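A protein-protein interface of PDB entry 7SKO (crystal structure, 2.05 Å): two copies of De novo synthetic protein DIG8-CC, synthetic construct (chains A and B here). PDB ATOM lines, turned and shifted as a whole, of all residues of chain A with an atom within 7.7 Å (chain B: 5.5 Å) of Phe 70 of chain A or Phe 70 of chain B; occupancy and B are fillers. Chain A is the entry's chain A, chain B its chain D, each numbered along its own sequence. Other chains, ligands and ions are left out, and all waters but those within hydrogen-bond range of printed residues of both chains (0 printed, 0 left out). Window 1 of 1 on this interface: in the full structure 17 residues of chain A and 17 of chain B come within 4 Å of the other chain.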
ATOM      1  N   MET A   3      -1.178  -6.965  -4.175  1.00  0.00           N
ATOM      2  CA  MET A   3      -1.678  -5.613  -3.945  1.00  0.00           C
ATOM      3  C   MET A   3      -0.834  -4.935  -2.873  1.00  0.00           C
ATOM      4  O   MET A   3      -0.837  -5.356  -1.712  1.00  0.00           O
ATOM      5  CB  MET A   3      -3.147  -5.657  -3.537  1.00  0.00           C
ATOM      6  CG  MET A   3      -3.827  -4.298  -3.523  1.00  0.00           C
ATOM      7  SD  MET A   3      -3.958  -3.573  -5.168  1.00  0.00           S
ATOM      8  CE  MET A   3      -4.853  -4.861  -6.033  1.00  0.00           C
ATOM      9  N   ILE A   5      -0.671  -1.189  -2.348  1.00  0.00           N
ATOM     10  CA  ILE A   5      -1.399  -0.061  -1.775  1.00  0.00           C
ATOM     11  C   ILE A   5      -2.774   0.014  -2.422  1.00  0.00           C
ATOM     12  O   ILE A   5      -2.897  -0.102  -3.646  1.00  0.00           O
ATOM     13  CB  ILE A   5      -0.644   1.270  -1.965  1.00  0.00           C
ATOM     14  CG1 ILE A   5       0.752   1.192  -1.345  1.00  0.00           C
ATOM     15  CG2 ILE A   5      -1.428   2.426  -1.358  1.00  0.00           C
ATOM     16  CD1 ILE A   5       1.592   2.407  -1.607  1.00  0.00           C
ATOM     17  N   GLU A   6      -3.807   0.209  -1.604  1.00  0.00           N
ATOM     18  CA  GLU A   6      -5.171   0.393  -2.078  1.00  0.00           C
ATOM     19  C   GLU A   6      -5.727   1.680  -1.488  1.00  0.00           C
ATOM     20  O   GLU A   6      -5.701   1.865  -0.266  1.00  0.00           O
ATOM     21  CB  GLU A   6      -6.058  -0.795  -1.693  1.00  0.00           C
ATOM     22  CG  GLU A   6      -6.652  -1.542  -2.874  1.00  0.00           C
ATOM     23  CD  GLU A   6      -7.717  -2.537  -2.458  1.00  0.00           C
ATOM     24  OE1 GLU A   6      -7.354  -3.638  -1.993  1.00  0.00           O
ATOM     25  OE2 GLU A   6      -8.917  -2.218  -2.596  1.00  0.00           O
ATOM     26  N   VAL A   7      -6.227   2.563  -2.348  1.00  0.00           N
ATOM     27  CA  VAL A   7      -6.790   3.842  -1.931  1.00  0.00           C
ATOM     28  C   VAL A   7      -8.203   3.947  -2.484  1.00  0.00           C
ATOM     29  O   VAL A   7      -8.420   3.746  -3.685  1.00  0.00           O
ATOM     30  CB  VAL A   7      -5.931   5.030  -2.406  1.00  0.00           C
ATOM     31  CG1 VAL A   7      -6.620   6.348  -2.083  1.00  0.00           C
ATOM     32  CG2 VAL A   7      -4.552   4.976  -1.768  1.00  0.00           C
ATOM     33  N   ARG A   8      -9.160   4.261  -1.614  1.00  0.00           N
ATOM     34  CA  ARG A   8     -10.557   4.393  -2.002  1.00  0.00           C
ATOM     35  C   ARG A   8     -11.126   5.677  -1.420  1.00  0.00           C
ATOM     36  O   ARG A   8     -10.956   5.952  -0.227  1.00  0.00           O
ATOM     37  CB  ARG A   8     -11.376   3.185  -1.533  1.00  0.00           C
ATOM     38  CG  ARG A   8     -12.770   3.103  -2.133  1.00  0.00           C
ATOM     39  CD  ARG A   8     -13.465   1.811  -1.733  1.00  0.00           C
ATOM     40  NE  ARG A   8     -14.868   1.795  -2.127  1.00  0.00           N
ATOM     41  CZ  ARG A   8     -15.847   2.364  -1.437  1.00  0.00           C
ATOM     42  NH1 ARG A   8     -15.615   2.992  -0.296  1.00  0.00           N
ATOM     43  NH2 ARG A   8     -17.093   2.295  -1.901  1.00  0.00           N
ATOM     44  N   VAL A   9     -11.790   6.462  -2.264  1.00  0.00           N
ATOM     45  CA  VAL A   9     -12.474   7.684  -1.854  1.00  0.00           C
ATOM     46  C   VAL A   9     -13.923   7.571  -2.306  1.00  0.00           C
ATOM     47  O   VAL A   9     -14.197   7.495  -3.511  1.00  0.00           O
ATOM     48  CB  VAL A   9     -11.811   8.941  -2.442  1.00  0.00           C
ATOM     49  CG1 VAL A   9     -12.495  10.196  -1.922  1.00  0.00           C
ATOM     50  CG2 VAL A   9     -10.324   8.963  -2.114  1.00  0.00           C
ATOM     51  N   VAL A  14     -12.278   8.204   3.058  1.00  0.00           N
ATOM     52  CA  VAL A  14     -11.002   7.836   2.458  1.00  0.00           C
ATOM     53  C   VAL A  14     -10.478   6.595   3.162  1.00  0.00           C
ATOM     54  O   VAL A  14     -10.360   6.574   4.395  1.00  0.00           O
ATOM     55  CB  VAL A  14      -9.987   8.989   2.549  1.00  0.00           C
ATOM     56  CG1 VAL A  14      -8.626   8.537   2.041  1.00  0.00           C
ATOM     57  CG2 VAL A  14     -10.480  10.188   1.762  1.00  0.00           C
ATOM     58  N   ARG A  15     -10.166   5.561   2.387  1.00  0.00           N
ATOM     59  CA  ARG A  15      -9.625   4.317   2.913  1.00  0.00           C
ATOM     60  C   ARG A  15      -8.288   4.027   2.248  1.00  0.00           C
ATOM     61  O   ARG A  15      -8.189   4.028   1.017  1.00  0.00           O
ATOM     62  CB  ARG A  15     -10.593   3.153   2.687  1.00  0.00           C
ATOM     63  CG  ARG A  15     -11.732   3.097   3.690  1.00  0.00           C
ATOM     64  CD  ARG A  15     -12.729   2.008   3.334  1.00  0.00           C
ATOM     65  NE  ARG A  15     -13.842   1.970   4.274  1.00  0.00           N
ATOM     66  CZ  ARG A  15     -15.029   1.444   4.007  1.00  0.00           C
ATOM     67  NH1 ARG A  15     -15.295   0.898   2.833  1.00  0.00           N
ATOM     68  NH2 ARG A  15     -15.973   1.466   4.943  1.00  0.00           N
ATOM     69  N   VAL A  16      -7.266   3.781   3.065  1.00  0.00           N
ATOM     70  CA  VAL A  16      -5.933   3.432   2.589  1.00  0.00           C
ATOM     71  C   VAL A  16      -5.531   2.125   3.255  1.00  0.00           C
ATOM     72  O   VAL A  16      -5.479   2.045   4.489  1.00  0.00           O
ATOM     73  CB  VAL A  16      -4.900   4.531   2.893  1.00  0.00           C
ATOM     74  CG1 VAL A  16      -3.552   4.169   2.286  1.00  0.00           C
ATOM     75  CG2 VAL A  16      -5.381   5.877   2.371  1.00  0.00           C
ATOM     76  N   ARG A  27      -0.507  10.986   3.878  1.00  0.00           N
ATOM     77  CA  ARG A  27      -0.859  12.395   3.982  1.00  0.00           C
ATOM     78  C   ARG A  27      -2.119  12.638   3.163  1.00  0.00           C
ATOM     79  O   ARG A  27      -2.150  12.340   1.965  1.00  0.00           O
ATOM     80  CB  ARG A  27       0.288  13.284   3.495  1.00  0.00           C
ATOM     81  CG  ARG A  27       0.057  14.769   3.698  1.00  0.00           C
ATOM     82  CD  ARG A  27       1.333  15.562   3.461  1.00  0.00           C
ATOM     83  NE  ARG A  27       1.783  15.473   2.078  1.00  0.00           N
ATOM     84  CZ  ARG A  27       2.291  16.485   1.387  1.00  0.00           C
ATOM     85  NH1 ARG A  27       2.428  17.687   1.924  1.00  0.00           N
ATOM     86  NH2 ARG A  27       2.671  16.287   0.129  1.00  0.00           N
ATOM     87  N   THR A  29      -4.752  15.562   1.978  1.00  0.00           N
ATOM     88  CA  THR A  29      -4.930  16.999   1.816  1.00  0.00           C
ATOM     89  C   THR A  29      -6.255  17.265   1.117  1.00  0.00           C
ATOM     90  O   THR A  29      -6.521  16.706   0.048  1.00  0.00           O
ATOM     91  CB  THR A  29      -3.778  17.614   1.014  1.00  0.00           C
ATOM     92  OG1 THR A  29      -2.527  17.215   1.587  1.00  0.00           O
ATOM     93  CG2 THR A  29      -3.874  19.132   1.023  1.00  0.00           C
ATOM     94  N   ALA A  57      -9.673  16.003  -3.220  1.00  0.00           N
ATOM     95  CA  ALA A  57      -8.787  15.500  -2.183  1.00  0.00           C
ATOM     96  C   ALA A  57      -7.573  14.847  -2.824  1.00  0.00           C
ATOM     97  O   ALA A  57      -7.612  14.411  -3.979  1.00  0.00           O
ATOM     98  CB  ALA A  57      -9.504  14.504  -1.265  1.00  0.00           C
ATOM     99  N   GLU A  58      -6.490  14.781  -2.056  1.00  0.00           N
ATOM    100  CA  GLU A  58      -5.250  14.153  -2.490  1.00  0.00           C
ATOM    101  C   GLU A  58      -4.752  13.226  -1.393  1.00  0.00           C
ATOM    102  O   GLU A  58      -4.676  13.625  -0.227  1.00  0.00           O
ATOM    103  CB  GLU A  58      -4.181  15.199  -2.821  1.00  0.00           C
ATOM    104  CG  GLU A  58      -2.820  14.609  -3.147  1.00  0.00           C
ATOM    105  CD  GLU A  58      -1.718  15.647  -3.142  1.00  0.00           C
ATOM    106  OE1 GLU A  58      -1.742  16.544  -4.012  1.00  0.00           O
ATOM    107  OE2 GLU A  58      -0.827  15.569  -2.271  1.00  0.00           O
ATOM    108  N   VAL A  59      -4.415  11.995  -1.766  1.00  0.00           N
ATOM    109  CA  VAL A  59      -3.875  11.007  -0.841  1.00  0.00           C
ATOM    110  C   VAL A  59      -2.455  10.686  -1.278  1.00  0.00           C
ATOM    111  O   VAL A  59      -2.233  10.236  -2.410  1.00  0.00           O
ATOM    112  CB  VAL A  59      -4.737   9.736  -0.793  1.00  0.00           C
ATOM    113  CG1 VAL A  59      -4.132   8.725   0.170  1.00  0.00           C
ATOM    114  CG2 VAL A  59      -6.162  10.080  -0.388  1.00  0.00           C
ATOM    115  N   GLU A  60      -1.498  10.920  -0.386  1.00  0.00           N
ATOM    116  CA  GLU A  60      -0.088  10.662  -0.646  1.00  0.00           C
ATOM    117  C   GLU A  60       0.402   9.596   0.320  1.00  0.00           C
ATOM    118  O   GLU A  60       0.232   9.731   1.537  1.00  0.00           O
ATOM    119  CB  GLU A  60       0.740  11.940  -0.498  1.00  0.00           C
ATOM    120  CG  GLU A  60       2.093  11.892  -1.186  1.00  0.00           C
ATOM    121  CD  GLU A  60       2.985  13.052  -0.791  1.00  0.00           C
ATOM    122  OE1 GLU A  60       3.666  12.952   0.252  1.00  0.00           O
ATOM    123  OE2 GLU A  60       3.001  14.065  -1.520  1.00  0.00           O
ATOM    124  N   VAL A  61       1.007   8.541  -0.219  1.00  0.00           N
ATOM    125  CA  VAL A  61       1.492   7.416   0.571  1.00  0.00           C
ATOM    126  C   VAL A  61       3.000   7.320   0.393  1.00  0.00           C
ATOM    127  O   VAL A  61       3.497   7.287  -0.739  1.00  0.00           O
ATOM    128  CB  VAL A  61       0.807   6.099   0.167  1.00  0.00           C
ATOM    129  CG1 VAL A  61       1.215   4.979   1.112  1.00  0.00           C
ATOM    130  CG2 VAL A  61      -0.706   6.268   0.161  1.00  0.00           C
ATOM    131  N   LYS A  67       7.322   7.040  -2.987  1.00  0.00           N
ATOM    132  CA  LYS A  67       6.143   7.868  -2.776  1.00  0.00           C
ATOM    133  C   LYS A  67       5.095   7.549  -3.831  1.00  0.00           C
ATOM    134  O   LYS A  67       5.423   7.344  -5.005  1.00  0.00           O
ATOM    135  CB  LYS A  67       6.491   9.360  -2.821  1.00  0.00           C
ATOM    136  CG  LYS A  67       6.795   9.969  -1.461  1.00  0.00           C
ATOM    137  CD  LYS A  67       6.864  11.485  -1.541  1.00  0.00           C
ATOM    138  CE  LYS A  67       8.079  12.025  -0.806  1.00  0.00           C
ATOM    139  NZ  LYS A  67       8.816  13.030  -1.620  1.00  0.00           N
ATOM    140  N   TYR A  68       3.835   7.505  -3.407  1.00  0.00           N
ATOM    141  CA  TYR A  68       2.710   7.237  -4.292  1.00  0.00           C
ATOM    142  C   TYR A  68       1.624   8.268  -4.024  1.00  0.00           C
ATOM    143  O   TYR A  68       1.237   8.479  -2.871  1.00  0.00           O
ATOM    144  CB  TYR A  68       2.172   5.816  -4.090  1.00  0.00           C
ATOM    145  CG  TYR A  68       3.245   4.747  -4.136  1.00  0.00           C
ATOM    146  CD1 TYR A  68       3.977   4.419  -3.001  1.00  0.00           C
ATOM    147  CD2 TYR A  68       3.530   4.074  -5.316  1.00  0.00           C
ATOM    148  CE1 TYR A  68       4.957   3.446  -3.039  1.00  0.00           C
ATOM    149  CE2 TYR A  68       4.510   3.099  -5.364  1.00  0.00           C
ATOM    150  CZ  TYR A  68       5.220   2.790  -4.223  1.00  0.00           C
ATOM    151  OH  TYR A  68       6.196   1.821  -4.265  1.00  0.00           O
ATOM    152  N   ARG A  69       1.139   8.906  -5.086  1.00  0.00           N
ATOM    153  CA  ARG A  69       0.177   9.995  -4.978  1.00  0.00           C
ATOM    154  C   ARG A  69      -1.105   9.623  -5.708  1.00  0.00           C
ATOM    155  O   ARG A  69      -1.061   9.134  -6.842  1.00  0.00           O
ATOM    156  CB  ARG A  69       0.753  11.294  -5.550  1.00  0.00           C
ATOM    157  CG  ARG A  69      -0.152  12.503  -5.371  1.00  0.00           C
ATOM    158  CD  ARG A  69       0.566  13.794  -5.734  1.00  0.00           C
ATOM    159  NE  ARG A  69       1.575  14.157  -4.746  1.00  0.00           N
ATOM    160  CZ  ARG A  69       2.672  14.850  -5.018  1.00  0.00           C
ATOM    161  NH1 ARG A  69       2.941  15.268  -6.243  1.00  0.00           N
ATOM    162  NH2 ARG A  69       3.523  15.128  -4.034  1.00  0.00           N
ATOM    163  N   PHE A  70      -2.242   9.858  -5.057  1.00  0.00           N
ATOM    164  CA  PHE A  70      -3.553   9.630  -5.648  1.00  0.00           C
ATOM    165  C   PHE A  70      -4.381  10.895  -5.487  1.00  0.00           C
ATOM    166  O   PHE A  70      -4.499  11.425  -4.377  1.00  0.00           O
ATOM    167  CB  PHE A  70      -4.253   8.435  -4.996  1.00  0.00           C
ATOM    168  CG  PHE A  70      -3.519   7.135  -5.172  1.00  0.00           C
ATOM    169  CD1 PHE A  70      -2.527   6.755  -4.280  1.00  0.00           C
ATOM    170  CD2 PHE A  70      -3.804   6.302  -6.240  1.00  0.00           C
ATOM    171  CE1 PHE A  70      -1.848   5.560  -4.445  1.00  0.00           C
ATOM    172  CE2 PHE A  70      -3.129   5.109  -6.410  1.00  0.00           C
ATOM    173  CZ  PHE A  70      -2.149   4.738  -5.513  1.00  0.00           C
ATOM    174  N   GLN A  71      -4.953  11.376  -6.589  1.00  0.00           N
ATOM    175  CA  GLN A  71      -5.637  12.662  -6.616  1.00  0.00           C
ATOM    176  C   GLN A  71      -7.040  12.502  -7.176  1.00  0.00           C
ATOM    177  O   GLN A  71      -7.229  11.874  -8.222  1.00  0.00           O
ATOM    178  CB  GLN A  71      -4.859  13.679  -7.458  1.00  0.00           C
ATOM    179  CG  GLN A  71      -3.828  14.477  -6.681  1.00  0.00           C
ATOM    180  CD  GLN A  71      -3.264  15.629  -7.487  1.00  0.00           C
ATOM    181  OE1 GLN A  71      -2.102  15.608  -7.891  1.00  0.00           O
ATOM    182  NE2 GLN A  71      -4.089  16.641  -7.729  1.00  0.00           N
ATOM    183  N   LEU A  72      -8.018  13.075  -6.480  1.00  0.00           N
ATOM    184  CA  LEU A  72      -9.388  13.185  -6.967  1.00  0.00           C
ATOM    185  C   LEU A  72      -9.670  14.671  -7.161  1.00  0.00           C
ATOM    186  O   LEU A  72      -9.712  15.432  -6.189  1.00  0.00           O
ATOM    187  CB  LEU A  72     -10.376  12.550  -5.988  1.00  0.00           C
ATOM    188  CG  LEU A  72     -11.882  12.785  -6.162  1.00  0.00           C
ATOM    189  CD1 LEU A  72     -12.310  12.749  -7.631  1.00  0.00           C
ATOM    190  CD2 LEU A  72     -12.678  11.779  -5.345  1.00  0.00           C
ATOM    191  N   GLY A  73      -9.852  15.082  -8.411  1.00  0.00           N
ATOM    192  CA  GLY A  73     -10.077  16.482  -8.721  1.00  0.00           C
ATOM    193  C   GLY A  73      -8.803  17.216  -9.098  1.00  0.00           C
ATOM    194  O   GLY A  73      -7.724  16.625  -9.147  1.00  0.00           O
ATOM    195  OXT GLY A  73      -8.817  18.416  -9.370  1.00  0.00           O
ATOM    196  N   VAL B   7      -1.563   8.906  -9.765  1.00  0.00           N
ATOM    197  CA  VAL B   7      -2.860   8.732 -10.404  1.00  0.00           C
ATOM    198  C   VAL B   7      -3.725   9.935 -10.062  1.00  0.00           C
ATOM    199  O   VAL B   7      -3.914  10.253  -8.884  1.00  0.00           O
ATOM    200  CB  VAL B   7      -3.552   7.427  -9.963  1.00  0.00           C
ATOM    201  CG1 VAL B   7      -4.905   7.295 -10.643  1.00  0.00           C
ATOM    202  CG2 VAL B   7      -2.672   6.225 -10.275  1.00  0.00           C
ATOM    203  N   ARG B   8      -4.248  10.600 -11.090  1.00  0.00           N
ATOM    204  CA  ARG B   8      -5.106  11.763 -10.910  1.00  0.00           C
ATOM    205  C   ARG B   8      -6.356  11.599 -11.758  1.00  0.00           C
ATOM    206  O   ARG B   8      -6.267  11.284 -12.949  1.00  0.00           O
ATOM    207  CB  ARG B   8      -4.375  13.056 -11.285  1.00  0.00           C
ATOM    208  N   VAL B   9      -7.516  11.807 -11.141  1.00  0.00           N
ATOM    209  CA  VAL B   9      -8.802  11.788 -11.828  1.00  0.00           C
ATOM    210  C   VAL B   9      -9.471  13.132 -11.580  1.00  0.00           C
ATOM    211  O   VAL B   9      -9.810  13.458 -10.435  1.00  0.00           O
ATOM    212  CB  VAL B   9      -9.694  10.633 -11.346  1.00  0.00           C
ATOM    213  CG1 VAL B   9     -10.967  10.562 -12.179  1.00  0.00           C
ATOM    214  CG2 VAL B   9      -8.938   9.314 -11.409  1.00  0.00           C
ATOM    215  N   ALA B  57     -15.357   5.300 -11.097  1.00  0.00           N
ATOM    216  CA  ALA B  57     -14.285   4.635 -11.822  1.00  0.00           C
ATOM    217  C   ALA B  57     -13.330   3.943 -10.856  1.00  0.00           C
ATOM    218  O   ALA B  57     -13.358   4.163  -9.642  1.00  0.00           O
ATOM    219  CB  ALA B  57     -13.521   5.636 -12.696  1.00  0.00           C
ATOM    220  N   GLU B  58     -12.478   3.092 -11.423  1.00  0.00           N
ATOM    221  CA  GLU B  58     -11.432   2.402 -10.679  1.00  0.00           C
ATOM    222  C   GLU B  58     -10.193   2.306 -11.553  1.00  0.00           C
ATOM    223  O   GLU B  58     -10.288   1.938 -12.728  1.00  0.00           O
ATOM    224  CB  GLU B  58     -11.885   1.003 -10.244  1.00  0.00           C
ATOM    225  CG  GLU B  58     -10.815   0.203  -9.518  1.00  0.00           C
ATOM    226  CD  GLU B  58     -11.119  -1.283  -9.485  1.00  0.00           C
ATOM    227  OE1 GLU B  58     -12.308  -1.644  -9.345  1.00  0.00           O
ATOM    228  OE2 GLU B  58     -10.173  -2.090  -9.600  1.00  0.00           O
ATOM    229  N   VAL B  59      -9.039   2.639 -10.983  1.00  0.00           N
ATOM    230  CA  VAL B  59      -7.763   2.598 -11.690  1.00  0.00           C
ATOM    231  C   VAL B  59      -6.855   1.610 -10.973  1.00  0.00           C
ATOM    232  O   VAL B  59      -6.617   1.739  -9.766  1.00  0.00           O
ATOM    233  CB  VAL B  59      -7.107   3.985 -11.769  1.00  0.00           C
ATOM    234  CG1 VAL B  59      -5.766   3.895 -12.480  1.00  0.00           C
ATOM    235  CG2 VAL B  59      -8.027   4.967 -12.478  1.00  0.00           C
ATOM    236  N   GLU B  60      -6.347   0.631 -11.717  1.00  0.00           N
ATOM    237  CA  GLU B  60      -5.442  -0.380 -11.185  1.00  0.00           C
ATOM    238  C   GLU B  60      -4.148  -0.359 -11.983  1.00  0.00           C
ATOM    239  O   GLU B  60      -4.171  -0.482 -13.212  1.00  0.00           O
ATOM    240  CB  GLU B  60      -6.082  -1.770 -11.237  1.00  0.00           C
ATOM    241  CG  GLU B  60      -5.354  -2.826 -10.421  1.00  0.00           C
ATOM    242  CD  GLU B  60      -6.166  -4.095 -10.259  1.00  0.00           C
ATOM    243  OE1 GLU B  60      -7.146  -4.082  -9.484  1.00  0.00           O
ATOM    244  OE2 GLU B  60      -5.825  -5.107 -10.909  1.00  0.00           O
ATOM    245  N   TYR B  68      -1.301  -1.697  -7.512  1.00  0.00           N
ATOM    246  CA  TYR B  68      -1.784  -0.507  -6.825  1.00  0.00           C
ATOM    247  C   TYR B  68      -3.154  -0.155  -7.383  1.00  0.00           C
ATOM    248  O   TYR B  68      -3.322  -0.062  -8.604  1.00  0.00           O
ATOM    249  CB  TYR B  68      -0.811   0.668  -6.994  1.00  0.00           C
ATOM    250  CG  TYR B  68       0.630   0.322  -6.684  1.00  0.00           C
ATOM    251  CD1 TYR B  68       1.446  -0.275  -7.637  1.00  0.00           C
ATOM    252  CD2 TYR B  68       1.175   0.591  -5.435  1.00  0.00           C
ATOM    253  CE1 TYR B  68       2.761  -0.594  -7.357  1.00  0.00           C
ATOM    254  CE2 TYR B  68       2.491   0.277  -5.144  1.00  0.00           C
ATOM    255  CZ  TYR B  68       3.278  -0.315  -6.109  1.00  0.00           C
ATOM    256  OH  TYR B  68       4.587  -0.630  -5.826  1.00  0.00           O
ATOM    257  N   ARG B  69      -4.127   0.038  -6.498  1.00  0.00           N
ATOM    258  CA  ARG B  69      -5.514   0.242  -6.891  1.00  0.00           C
ATOM    259  C   ARG B  69      -6.035   1.557  -6.328  1.00  0.00           C
ATOM    260  O   ARG B  69      -5.785   1.890  -5.164  1.00  0.00           O
ATOM    261  CB  ARG B  69      -6.394  -0.921  -6.415  1.00  0.00           C
ATOM    262  CG  ARG B  69      -7.870  -0.772  -6.749  1.00  0.00           C
ATOM    263  CD  ARG B  69      -8.681  -1.918  -6.164  1.00  0.00           C
ATOM    264  NE  ARG B  69      -8.345  -3.194  -6.785  1.00  0.00           N
ATOM    265  CZ  ARG B  69      -8.488  -4.375  -6.198  1.00  0.00           C
ATOM    266  NH1 ARG B  69      -8.959  -4.482  -4.966  1.00  0.00           N
ATOM    267  NH2 ARG B  69      -8.152  -5.475  -6.865  1.00  0.00           N
ATOM    268  N   PHE B  70      -6.762   2.298  -7.164  1.00  0.00           N
ATOM    269  CA  PHE B  70      -7.358   3.578  -6.791  1.00  0.00           C
ATOM    270  C   PHE B  70      -8.820   3.557  -7.218  1.00  0.00           C
ATOM    271  O   PHE B  70      -9.119   3.594  -8.417  1.00  0.00           O
ATOM    272  CB  PHE B  70      -6.612   4.742  -7.447  1.00  0.00           C
ATOM    273  CG  PHE B  70      -7.075   6.099  -6.992  1.00  0.00           C
ATOM    274  CD1 PHE B  70      -7.391   6.330  -5.663  1.00  0.00           C
ATOM    275  CD2 PHE B  70      -7.175   7.148  -7.891  1.00  0.00           C
ATOM    276  CE1 PHE B  70      -7.810   7.579  -5.242  1.00  0.00           C
ATOM    277  CE2 PHE B  70      -7.592   8.400  -7.476  1.00  0.00           C
ATOM    278  CZ  PHE B  70      -7.909   8.614  -6.149  1.00  0.00           C
ATOM    279  N   GLN B  71      -9.726   3.493  -6.248  1.00  0.00           N
ATOM    280  CA  GLN B  71     -11.157   3.406  -6.509  1.00  0.00           C
ATOM    281  C   GLN B  71     -11.832   4.711  -6.107  1.00  0.00           C
ATOM    282  O   GLN B  71     -11.561   5.249  -5.029  1.00  0.00           O
ATOM    283  CB  GLN B  71     -11.780   2.230  -5.753  1.00  0.00           C
ATOM    284  CG  GLN B  71     -13.295   2.152  -5.861  1.00  0.00           C
ATOM    285  CD  GLN B  71     -13.760   1.014  -6.749  1.00  0.00           C
ATOM    286  OE1 GLN B  71     -13.006   0.083  -7.031  1.00  0.00           O
ATOM    287  NE2 GLN B  71     -15.008   1.086  -7.199  1.00  0.00           N
ATOM    288  N   LEU B  72     -12.706   5.213  -6.974  1.00  0.00           N
ATOM    289  CA  LEU B  72     -13.462   6.428  -6.692  1.00  0.00           C
ATOM    290  C   LEU B  72     -14.904   6.098  -6.327  1.00  0.00           C
ATOM    291  O   LEU B  72     -15.599   5.407  -7.074  1.00  0.00           O
ATOM    292  CB  LEU B  72     -13.428   7.379  -7.893  1.00  0.00           C
ATOM    293  CG  LEU B  72     -12.083   8.022  -8.240  1.00  0.00           C
ATOM    294  CD1 LEU B  72     -11.288   8.314  -6.978  1.00  0.00           C
ATOM    295  CD2 LEU B  72     -11.285   7.145  -9.194  1.00  0.00           C
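The backbone carbonyl oxygen (O) of Val 9 of chain B sits at hydrogen-bond distance from the backbone NH (N) of Gly 73 of chain A (2.6 Å).
The backbone carbonyl oxygen of Val 7 of chain B is in hydrogen-bond range of the backbone NH of Gln 71 of chain A (2.8 Å).
OH of Tyr 68 of chain A sits at hydrogen-bond distance from OH of Tyr 68 of chain B, at 3.3 Å.
N of Val 7 of chain A lies within hydrogen-bond range of O of Arg 69 of chain B, at 2.9 Å.
The guanidinium group of Arg 69 of chain B lies within salt-bridge range of the side-chain carboxylate of Glu 6 of chain A, at 3.3 Å.
The backbone carbonyl oxygen of Ile 5 of chain A lies within hydrogen-bond range of the backbone NH of Arg 69 of chain B (3.1 Å).
O of Arg 69 of chain A sits at hydrogen-bond distance from N of Val 7 of chain B (3.0 Å).
O of Val 7 of chain A lies within hydrogen-bond range of N of Gln 71 of chain B, at 2.9 Å.
The backbone carbonyl oxygen (O) of Gln 71 of chain A lies within hydrogen-bond range of the backbone NH (N) of Val 9 of chain B, 2.9 Å away.
The backbone carbonyl oxygen (O) of Gln 71 of chain B is in hydrogen-bond range of the backbone NH (N) of Val 9 of chain A (3.0 Å).
The side-chain carboxylate of Glu 58 of chain A lies within salt-bridge range of the guanidinium group of Arg 69 of chain A (3.7 Å).
The side-chain carboxylate (OE1) of Glu 60 of chain B lies within salt-bridge range of the guanidinium group (NE) of Arg 69 of chain B (3.1 Å).
OE2 of Glu 60 of chain A is in salt-bridge range of NH2 of Arg 69 of chain A, 2.8 Å away.
O of Val 59 of chain B sits at hydrogen-bond distance from N of Phe 70 of chain B (2.7 Å).
The side-chain carboxylate (OE1) of Glu 58 of chain B lies close to the side-chain amide oxygen (OE1) of Gln 71 of chain B.
Among the printed residues, pairs that only touch across the chains: Met 3 of chain A with Arg 69 of chain B, Ile 5 of chain A with Tyr 68 of chain B, Val 7 of chain A with Phe 70 of chain B, Arg 8 of chain A with Gln 71 of chain B, Val 9 of chain A with Leu 72 of chain B, Phe 70 of chain A with Val 7 of chain B, Phe 70 of chain A with Phe 70 of chain B, Gln 71 of chain A with Arg 8 of chain B, Gln 71 of chain A with Phe 70 of chain B and Leu 72 of chain A with Val 9 of chain B.
Of the printed residues of chain B, Ile 5 of chain A touches Tyr 68 (3.4 Å) and Arg 69 (3.1 Å).
Printed residues of chain B within 4 Å of Glu 6 of chain A: Arg 69 (3.3 Å).
Printed residues of chain B within 4 Å of Val 9 of chain A: Gln 71 and Leu 72.
Val 16 of chain A touches none of the printed residues of chain B.
Thr 29 of chain A touches none of the printed residues of chain B.
Of the printed residues of chain B, Arg 69 of chain A touches Val 7 (3.0 Å).
Phe 70 of chain A touches just these residues of chain B: Val 7 (3.3 Å) and Phe 70 (3.4 Å).
Of the printed residues of chain A, Tyr 68 of chain B touches Ile 5 and Tyr 68.
Of the printed residues of chain A, Phe 70 of chain B touches Val 7, Phe 70 and Gln 71.
The nearest residue of chain B that does not touch Phe 70 of chain A is Arg 69 of chain B (4.4 Å).
The nearest residue of chain A that does not touch Phe 70 of chain B is Val 9 of chain A (4.2 Å).
Hydrophobic or aromatic side chains of chain A within 4 Å of the printed part of chain B: Met 3, Ile 5, Val 7, Tyr 68, Phe 70 and Leu 72.
Of the 12 printed residues of chain B, 8 touch a printed residue of chain A.
Printed residues of chain B that touch a printed residue of chain A: Val 7, Arg 8, Val 9, Tyr 68, Arg 69, Phe 70, Gln 71 and Leu 72.
Among the printed residues, 20 pairs touch across the chains.
Val 7 of chain A touches Arg 69 of chain B, and with the chains exchanged Arg 69 of chain A touches Val 7 of chain B.
Val 7 of chain A touches Gln 71 of chain B, and with the chains exchanged Gln 71 of chain A touches Val 7 of chain B.
Phe 70 of chain A touches its own counterpart, Phe 70 of chain B.
Gln 71 of chain A touches Phe 70 of chain B, but with the chains exchanged Phe 70 of chain A does not touch Gln 71 of chain B (6.6 Å).
12 positions are printed for both chains.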
